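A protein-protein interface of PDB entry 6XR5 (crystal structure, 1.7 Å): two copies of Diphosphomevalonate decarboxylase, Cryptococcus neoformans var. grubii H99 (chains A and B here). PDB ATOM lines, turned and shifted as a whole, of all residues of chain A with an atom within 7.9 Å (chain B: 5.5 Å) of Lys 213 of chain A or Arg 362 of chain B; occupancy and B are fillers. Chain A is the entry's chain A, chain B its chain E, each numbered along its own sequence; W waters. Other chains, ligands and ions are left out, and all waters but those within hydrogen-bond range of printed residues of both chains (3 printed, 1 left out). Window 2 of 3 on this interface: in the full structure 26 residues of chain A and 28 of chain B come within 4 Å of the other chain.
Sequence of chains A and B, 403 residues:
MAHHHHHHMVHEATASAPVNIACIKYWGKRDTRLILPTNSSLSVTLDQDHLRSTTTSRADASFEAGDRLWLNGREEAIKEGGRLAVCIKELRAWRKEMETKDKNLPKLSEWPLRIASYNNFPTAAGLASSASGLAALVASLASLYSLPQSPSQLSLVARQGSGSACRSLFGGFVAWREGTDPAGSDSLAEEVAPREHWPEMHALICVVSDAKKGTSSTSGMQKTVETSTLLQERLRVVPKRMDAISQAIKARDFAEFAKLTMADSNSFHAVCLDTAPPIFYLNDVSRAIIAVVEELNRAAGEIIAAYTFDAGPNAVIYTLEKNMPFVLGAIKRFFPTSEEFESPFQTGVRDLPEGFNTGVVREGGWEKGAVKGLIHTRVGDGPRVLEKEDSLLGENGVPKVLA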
ATOM      1  N   SER A 209     -17.109 -13.110 -11.459  1.00  0.00           N
ATOM      2  CA  SER A 209     -18.046 -13.591 -10.452  1.00  0.00           C
ATOM      3  C   SER A 209     -18.257 -15.090 -10.613  1.00  0.00           C
ATOM      4  O   SER A 209     -18.317 -15.610 -11.726  1.00  0.00           O
ATOM      5  CB  SER A 209     -19.378 -12.844 -10.572  1.00  0.00           C
ATOM      6  OG  SER A 209     -20.356 -13.425  -9.715  1.00  0.00           O
ATOM      7  N   ASP A 210     -18.352 -15.802  -9.498  1.00  0.00           N
ATOM      8  CA  ASP A 210     -18.429 -17.264  -9.567  1.00  0.00           C
ATOM      9  C   ASP A 210     -19.444 -17.794  -8.559  1.00  0.00           C
ATOM     10  O   ASP A 210     -19.216 -18.813  -7.901  1.00  0.00           O
ATOM     11  CB  ASP A 210     -17.040 -17.874  -9.341  1.00  0.00           C
ATOM     12  CG  ASP A 210     -16.927 -19.342  -9.797  1.00  0.00           C
ATOM     13  OD1 ASP A 210     -17.750 -19.830 -10.622  1.00  0.00           O
ATOM     14  OD2 ASP A 210     -15.969 -19.996  -9.321  1.00  0.00           O
ATOM     15  N   ALA A 211     -20.603 -17.132  -8.454  1.00  0.00           N
ATOM     16  CA  ALA A 211     -21.565 -17.401  -7.388  1.00  0.00           C
ATOM     17  C   ALA A 211     -22.655 -18.410  -7.757  1.00  0.00           C
ATOM     18  O   ALA A 211     -23.621 -18.549  -6.998  1.00  0.00           O
ATOM     19  CB  ALA A 211     -22.224 -16.092  -6.940  1.00  0.00           C
ATOM     20  N   LYS A 212     -22.541 -19.118  -8.882  1.00  0.00           N
ATOM     21  CA  LYS A 212     -23.586 -20.062  -9.278  1.00  0.00           C
ATOM     22  C   LYS A 212     -23.151 -21.522  -9.202  1.00  0.00           C
ATOM     23  O   LYS A 212     -23.950 -22.410  -9.527  1.00  0.00           O
ATOM     24  CB  LYS A 212     -24.094 -19.747 -10.695  1.00  0.00           C
ATOM     25  N   LYS A 213     -21.919 -21.800  -8.787  1.00  0.00           N
ATOM     26  CA  LYS A 213     -21.467 -23.167  -8.590  1.00  0.00           C
ATOM     27  C   LYS A 213     -21.817 -23.643  -7.177  1.00  0.00           C
ATOM     28  O   LYS A 213     -22.305 -22.887  -6.331  1.00  0.00           O
ATOM     29  CB  LYS A 213     -19.957 -23.275  -8.834  1.00  0.00           C
ATOM     30  CG  LYS A 213     -19.118 -22.474  -7.857  1.00  0.00           C
ATOM     31  CD  LYS A 213     -17.631 -22.688  -8.112  1.00  0.00           C
ATOM     32  CE  LYS A 213     -16.805 -22.295  -6.887  1.00  0.00           C
ATOM     33  NZ  LYS A 213     -17.245 -20.987  -6.317  1.00  0.00           N
ATOM     34  N   GLY A 214     -21.564 -24.917  -6.930  1.00  0.00           N
ATOM     35  CA  GLY A 214     -21.708 -25.493  -5.602  1.00  0.00           C
ATOM     36  C   GLY A 214     -20.365 -25.620  -4.919  1.00  0.00           C
ATOM     37  O   GLY A 214     -19.486 -24.760  -5.070  1.00  0.00           O
ATOM     38  N   THR A 215     -20.196 -26.719  -4.188  1.00  0.00           N
ATOM     39  CA  THR A 215     -18.953 -27.032  -3.489  1.00  0.00           C
ATOM     40  C   THR A 215     -18.604 -28.510  -3.642  1.00  0.00           C
ATOM     41  O   THR A 215     -19.364 -29.386  -3.221  1.00  0.00           O
ATOM     42  CB  THR A 215     -19.045 -26.684  -1.988  1.00  0.00           C
ATOM     43  OG1 THR A 215     -19.232 -25.269  -1.832  1.00  0.00           O
ATOM     44  CG2 THR A 215     -17.777 -27.108  -1.263  1.00  0.00           C
ATOM     45  N   PHE A 280     -14.479 -28.776 -13.170  1.00  0.00           N
ATOM     46  CA  PHE A 280     -14.936 -27.595 -13.902  1.00  0.00           C
ATOM     47  C   PHE A 280     -14.399 -26.326 -13.239  1.00  0.00           C
ATOM     48  O   PHE A 280     -14.637 -26.100 -12.043  1.00  0.00           O
ATOM     49  CB  PHE A 280     -16.462 -27.540 -13.918  1.00  0.00           C
ATOM     50  CG  PHE A 280     -17.120 -28.709 -14.599  1.00  0.00           C
ATOM     51  CD1 PHE A 280     -17.267 -28.720 -15.975  1.00  0.00           C
ATOM     52  CD2 PHE A 280     -17.607 -29.775 -13.863  1.00  0.00           C
ATOM     53  CE1 PHE A 280     -17.922 -29.810 -16.610  1.00  0.00           C
ATOM     54  CE2 PHE A 280     -18.255 -30.843 -14.493  1.00  0.00           C
ATOM     55  CZ  PHE A 280     -18.397 -30.851 -15.862  1.00  0.00           C
ATOM     56  N   TYR A 281     -13.729 -25.488 -14.020  1.00  0.00           N
ATOM     57  CA  TYR A 281     -13.204 -24.204 -13.563  1.00  0.00           C
ATOM     58  C   TYR A 281     -13.739 -23.035 -14.372  1.00  0.00           C
ATOM     59  O   TYR A 281     -14.116 -21.998 -13.795  1.00  0.00           O
ATOM     60  CB  TYR A 281     -11.669 -24.196 -13.660  1.00  0.00           C
ATOM     61  CG  TYR A 281     -11.032 -25.107 -12.626  1.00  0.00           C
ATOM     62  CD1 TYR A 281     -11.366 -24.994 -11.297  1.00  0.00           C
ATOM     63  CD2 TYR A 281     -10.064 -26.047 -13.005  1.00  0.00           C
ATOM     64  CE1 TYR A 281     -10.754 -25.806 -10.354  1.00  0.00           C
ATOM     65  CE2 TYR A 281      -9.447 -26.850 -12.057  1.00  0.00           C
ATOM     66  CZ  TYR A 281      -9.802 -26.724 -10.752  1.00  0.00           C
ATOM     67  OH  TYR A 281      -9.203 -27.544  -9.817  1.00  0.00           O
ATOM     68  N   ASN A 283     -16.414 -20.820 -16.237  1.00  0.00           N
ATOM     69  CA  ASN A 283     -17.867 -20.704 -16.143  1.00  0.00           C
ATOM     70  C   ASN A 283     -18.399 -19.922 -17.341  1.00  0.00           C
ATOM     71  O   ASN A 283     -17.641 -19.683 -18.277  1.00  0.00           O
ATOM     72  CB  ASN A 283     -18.292 -20.088 -14.793  1.00  0.00           C
ATOM     73  CG  ASN A 283     -17.897 -18.621 -14.617  1.00  0.00           C
ATOM     74  OD1 ASN A 283     -17.572 -17.902 -15.564  1.00  0.00           O
ATOM     75  ND2 ASN A 283     -17.952 -18.170 -13.374  1.00  0.00           N
ATOM     76  N   GLY A 312      -9.771 -21.790 -11.913  1.00  0.00           N
ATOM     77  CA  GLY A 312     -10.932 -21.016 -11.563  1.00  0.00           C
ATOM     78  C   GLY A 312     -11.317 -20.221 -12.793  1.00  0.00           C
ATOM     79  O   GLY A 312     -10.671 -20.319 -13.832  1.00  0.00           O
ATOM     80  N   PRO A 313     -12.385 -19.427 -12.698  1.00  0.00           N
ATOM     81  CA  PRO A 313     -12.923 -18.769 -13.892  1.00  0.00           C
ATOM     82  C   PRO A 313     -12.257 -17.458 -14.281  1.00  0.00           C
ATOM     83  O   PRO A 313     -12.608 -16.923 -15.342  1.00  0.00           O
ATOM     84  CB  PRO A 313     -14.395 -18.531 -13.504  1.00  0.00           C
ATOM     85  CG  PRO A 313     -14.306 -18.265 -12.001  1.00  0.00           C
ATOM     86  CD  PRO A 313     -13.199 -19.184 -11.498  1.00  0.00           C
ATOM     87  N   ARG B 287     -23.372 -28.024 -16.082  1.00  0.00           N
ATOM     88  CA  ARG B 287     -22.421 -28.404 -15.039  1.00  0.00           C
ATOM     89  C   ARG B 287     -23.131 -28.713 -13.727  1.00  0.00           C
ATOM     90  O   ARG B 287     -22.739 -29.653 -13.004  1.00  0.00           O
ATOM     91  CB  ARG B 287     -21.381 -27.295 -14.834  1.00  0.00           C
ATOM     92  CG  ARG B 287     -20.435 -27.571 -13.665  1.00  0.00           C
ATOM     93  CD  ARG B 287     -19.686 -26.302 -13.229  1.00  0.00           C
ATOM     94  NE  ARG B 287     -18.990 -26.480 -11.953  1.00  0.00           N
ATOM     95  CZ  ARG B 287     -18.137 -25.605 -11.422  1.00  0.00           C
ATOM     96  NH1 ARG B 287     -17.863 -24.472 -12.053  1.00  0.00           N
ATOM     97  NH2 ARG B 287     -17.560 -25.876 -10.258  1.00  0.00           N
ATOM     98  N   THR B 358     -26.482 -31.160  -0.230  1.00  0.00           N
ATOM     99  CA  THR B 358     -27.051 -30.125  -1.086  1.00  0.00           C
ATOM    100  C   THR B 358     -26.040 -29.040  -1.420  1.00  0.00           C
ATOM    101  O   THR B 358     -26.335 -28.197  -2.275  1.00  0.00           O
ATOM    102  CB  THR B 358     -28.293 -29.498  -0.442  1.00  0.00           C
ATOM    103  OG1 THR B 358     -27.957 -28.947   0.837  1.00  0.00           O
ATOM    104  CG2 THR B 358     -29.406 -30.533  -0.294  1.00  0.00           C
ATOM    105  N   GLY B 359     -24.859 -29.071  -0.791  1.00  0.00           N
ATOM    106  CA  GLY B 359     -23.795 -28.138  -1.096  1.00  0.00           C
ATOM    107  C   GLY B 359     -23.239 -28.278  -2.494  1.00  0.00           C
ATOM    108  O   GLY B 359     -22.572 -27.363  -2.972  1.00  0.00           O
ATOM    109  N   VAL B 360     -23.502 -29.399  -3.168  1.00  0.00           N
ATOM    110  CA  VAL B 360     -22.988 -29.560  -4.524  1.00  0.00           C
ATOM    111  C   VAL B 360     -23.689 -28.647  -5.511  1.00  0.00           C
ATOM    112  O   VAL B 360     -23.224 -28.523  -6.652  1.00  0.00           O
ATOM    113  CB  VAL B 360     -23.098 -31.003  -5.044  1.00  0.00           C
ATOM    114  CG1 VAL B 360     -22.370 -31.967  -4.101  1.00  0.00           C
ATOM    115  CG2 VAL B 360     -24.572 -31.416  -5.238  1.00  0.00           C
ATOM    116  N   VAL B 361     -24.781 -28.016  -5.095  1.00  0.00           N
ATOM    117  CA  VAL B 361     -25.519 -27.037  -5.884  1.00  0.00           C
ATOM    118  C   VAL B 361     -25.457 -25.695  -5.173  1.00  0.00           C
ATOM    119  O   VAL B 361     -25.441 -25.622  -3.940  1.00  0.00           O
ATOM    120  CB  VAL B 361     -26.995 -27.465  -6.078  1.00  0.00           C
ATOM    121  CG1 VAL B 361     -27.774 -26.443  -6.918  1.00  0.00           C
ATOM    122  CG2 VAL B 361     -27.059 -28.826  -6.703  1.00  0.00           C
ATOM    123  N   ARG B 362     -25.446 -24.622  -5.965  1.00  0.00           N
ATOM    124  CA  ARG B 362     -25.549 -23.281  -5.405  1.00  0.00           C
ATOM    125  C   ARG B 362     -26.701 -23.209  -4.405  1.00  0.00           C
ATOM    126  O   ARG B 362     -27.729 -23.883  -4.548  1.00  0.00           O
ATOM    127  CB  ARG B 362     -25.754 -22.250  -6.519  1.00  0.00           C
ATOM    128  CG  ARG B 362     -27.076 -22.456  -7.275  1.00  0.00           C
ATOM    129  CD  ARG B 362     -27.176 -21.566  -8.497  1.00  0.00           C
ATOM    130  NE  ARG B 362     -27.737 -20.263  -8.169  1.00  0.00           N
ATOM    131  CZ  ARG B 362     -28.167 -19.390  -9.074  1.00  0.00           C
ATOM    132  NH1 ARG B 362     -28.077 -19.677 -10.365  1.00  0.00           N
ATOM    133  NH2 ARG B 362     -28.684 -18.233  -8.689  1.00  0.00           N
ATOM    134  N   GLU B 363     -26.505 -22.403  -3.367  1.00  0.00           N
ATOM    135  CA  GLU B 363     -27.508 -22.264  -2.318  1.00  0.00           C
ATOM    136  C   GLU B 363     -28.850 -21.849  -2.908  1.00  0.00           C
ATOM    137  O   GLU B 363     -28.933 -20.919  -3.722  1.00  0.00           O
ATOM    138  CB  GLU B 363     -27.041 -21.244  -1.276  1.00  0.00           C
ATOM    139  CG  GLU B 363     -27.831 -21.277   0.028  1.00  0.00           C
ATOM    140  CD  GLU B 363     -29.200 -20.624  -0.099  1.00  0.00           C
ATOM    141  OE1 GLU B 363     -29.271 -19.501  -0.647  1.00  0.00           O
ATOM    142  OE2 GLU B 363     -30.206 -21.233   0.330  1.00  0.00           O
ATOM    143  N   GLY B 364     -29.902 -22.551  -2.495  1.00  0.00           N
ATOM    144  CA  GLY B 364     -31.240 -22.258  -2.944  1.00  0.00           C
ATOM    145  C   GLY B 364     -31.586 -22.810  -4.305  1.00  0.00           C
ATOM    146  O   GLY B 364     -32.735 -22.657  -4.741  1.00  0.00           O
ATOM    147  N   GLY B 365     -30.639 -23.455  -4.981  1.00  0.00           N
ATOM    148  CA  GLY B 365     -30.882 -24.000  -6.299  1.00  0.00           C
ATOM    149  C   GLY B 365     -30.953 -22.913  -7.357  1.00  0.00           C
ATOM    150  O   GLY B 365     -30.541 -21.772  -7.155  1.00  0.00           O
ATOM    151  N   TRP B 366     -31.505 -23.292  -8.502  1.00  0.00           N
ATOM    152  CA  TRP B 366     -31.513 -22.459  -9.699  1.00  0.00           C
ATOM    153  C   TRP B 366     -32.866 -21.790  -9.899  1.00  0.00           C
ATOM    154  O   TRP B 366     -33.882 -22.240  -9.377  1.00  0.00           O
ATOM    155  CB  TRP B 366     -31.145 -23.314 -10.904  1.00  0.00           C
ATOM    156  CG  TRP B 366     -29.686 -23.562 -10.921  1.00  0.00           C
ATOM    157  CD1 TRP B 366     -28.965 -24.447 -10.143  1.00  0.00           C
ATOM    158  CD2 TRP B 366     -28.741 -22.868 -11.727  1.00  0.00           C
ATOM    159  NE1 TRP B 366     -27.616 -24.340 -10.446  1.00  0.00           N
ATOM    160  CE2 TRP B 366     -27.462 -23.370 -11.413  1.00  0.00           C
ATOM    161  CE3 TRP B 366     -28.856 -21.855 -12.687  1.00  0.00           C
ATOM    162  CZ2 TRP B 366     -26.306 -22.913 -12.054  1.00  0.00           C
ATOM    163  CZ3 TRP B 366     -27.704 -21.390 -13.305  1.00  0.00           C
ATOM    164  CH2 TRP B 366     -26.452 -21.924 -12.991  1.00  0.00           C
ATOM    165  N   GLU B 367     -32.859 -20.677 -10.641  1.00  0.00           N
ATOM    166  CA  GLU B 367     -34.092 -19.957 -10.920  1.00  0.00           C
ATOM    167  C   GLU B 367     -35.045 -20.826 -11.738  1.00  0.00           C
ATOM    168  O   GLU B 367     -34.622 -21.703 -12.492  1.00  0.00           O
ATOM    169  CB  GLU B 367     -33.773 -18.657 -11.665  1.00  0.00           C
ATOM    170  CG  GLU B 367     -32.879 -17.680 -10.875  1.00  0.00           C
ATOM    171  CD  GLU B 367     -31.359 -17.996 -10.869  1.00  0.00           C
ATOM    172  OE1 GLU B 367     -30.894 -19.052 -11.365  1.00  0.00           O
ATOM    173  OE2 GLU B 367     -30.610 -17.151 -10.337  1.00  0.00           O
HETATM  174  O   HOH W   1     -16.215 -22.137 -12.000  1.00  0.00           O
HETATM  175  O   HOH W   2     -25.162 -24.888  -8.897  1.00  0.00           O
HETATM  176  O   HOH W   3     -21.554 -25.249  -0.690  1.00  0.00           O
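The backbone carbonyl oxygen (O) of Gly 359 of chain B sits at hydrogen-bond distance from the backbone NH (N) of Thr 215 of chain A, 2.7 Å away.
O of Phe 280 of chain A sits at hydrogen-bond distance from NH2 of Arg 287 of chain B (3.4 Å).
Lys 212 of chain A touches Arg 362 of chain B.
O of Lys 212 of chain A touches CZ2 of Trp 366 of chain B, at 3.5 Å.
Lys 213 of chain A touches Arg 287 of chain B (CB to NH2, 3.8 Å).
Lys 213 of chain A touches Arg 362 of chain B.
Gly 214 of chain A touches Gly 359 of chain B.
Gly 214 of chain A touches Val 360 of chain B.
Val 361 of chain B touches Gly 214 of chain A (C to CA, 3.8 Å).
N of Arg 362 of chain B touches CA of Gly 214 of chain A (3.9 Å).
Thr 215 of chain A touches Val 360 of chain B.
Of the 12 printed residues of chain A, 5 touch a printed residue of chain B.
Printed residues of chain A that touch a printed residue of chain B: Lys 212, Lys 213, Gly 214, Thr 215 and Phe 280.
Of the 11 printed residues of chain B, 6 touch a printed residue of chain A.
Printed residues of chain B that touch a printed residue of chain A: Arg 287, Gly 359, Val 360, Val 361, Arg 362 and Trp 366.
Hydrophobic or aromatic side chains of chain B that line the printed part of chain A: Trp 366.
Among the printed residues, 11 pairs touch across the chains.
No position is printed for both chains.
Of the 11 pairs that touch across the chains among the printed residues, none has its exchanged pair printed and touching as well.
OD2 of Asp 210 of chain A is in salt-bridge range of NZ of Lys 213 of chain A, 3.4 Å away.
O of Gly 365 of chain B lies within hydrogen-bond range of NE of Arg 362 of chain B, at 3.3 Å.
The guanidinium group (NH2) of Arg 362 of chain B lies within salt-bridge range of the side-chain carboxylate (OE2) of Glu 367 of chain B (2.8 Å).
Water W3 bridges the side-chain hydroxyl (OG1) of Thr 215 of chain A and the backbone carbonyl oxygen (O) of Gly 359 of chain B.
Water W1 lies within hydrogen-bond range of O of Tyr 281 of chain A (2.8 Å), NH1 of Arg 287 of chain B (2.9 Å) and OD1 of Asp 210 of chain A (3.1 Å).
Water W2 lies within hydrogen-bond range of O of Lys 212 of chain A, NE1 of Trp 366 of chain B and N of Arg 362 of chain B.
Of the printed residues of chain B, Lys 212 of chain A touches Arg 362 (3.5 Å) and Trp 366 (3.5 Å).
Printed residues of chain B within 4 Å of Lys 213 of chain A: Arg 287 and Arg 362.
Asn 283 of chain A touches none of the printed residues of chain B.
Printed residues of chain A within 4 Å of Val 361 of chain B: Gly 214.
Arg 362 of chain B touches three residues of chain A.
Of the printed residues of chain A, Trp 366 of chain B touches Lys 212 (3.5 Å).
The nearest residue of chain A that does not touch Arg 362 of chain B is Ala 211 of chain A (4.3 Å).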
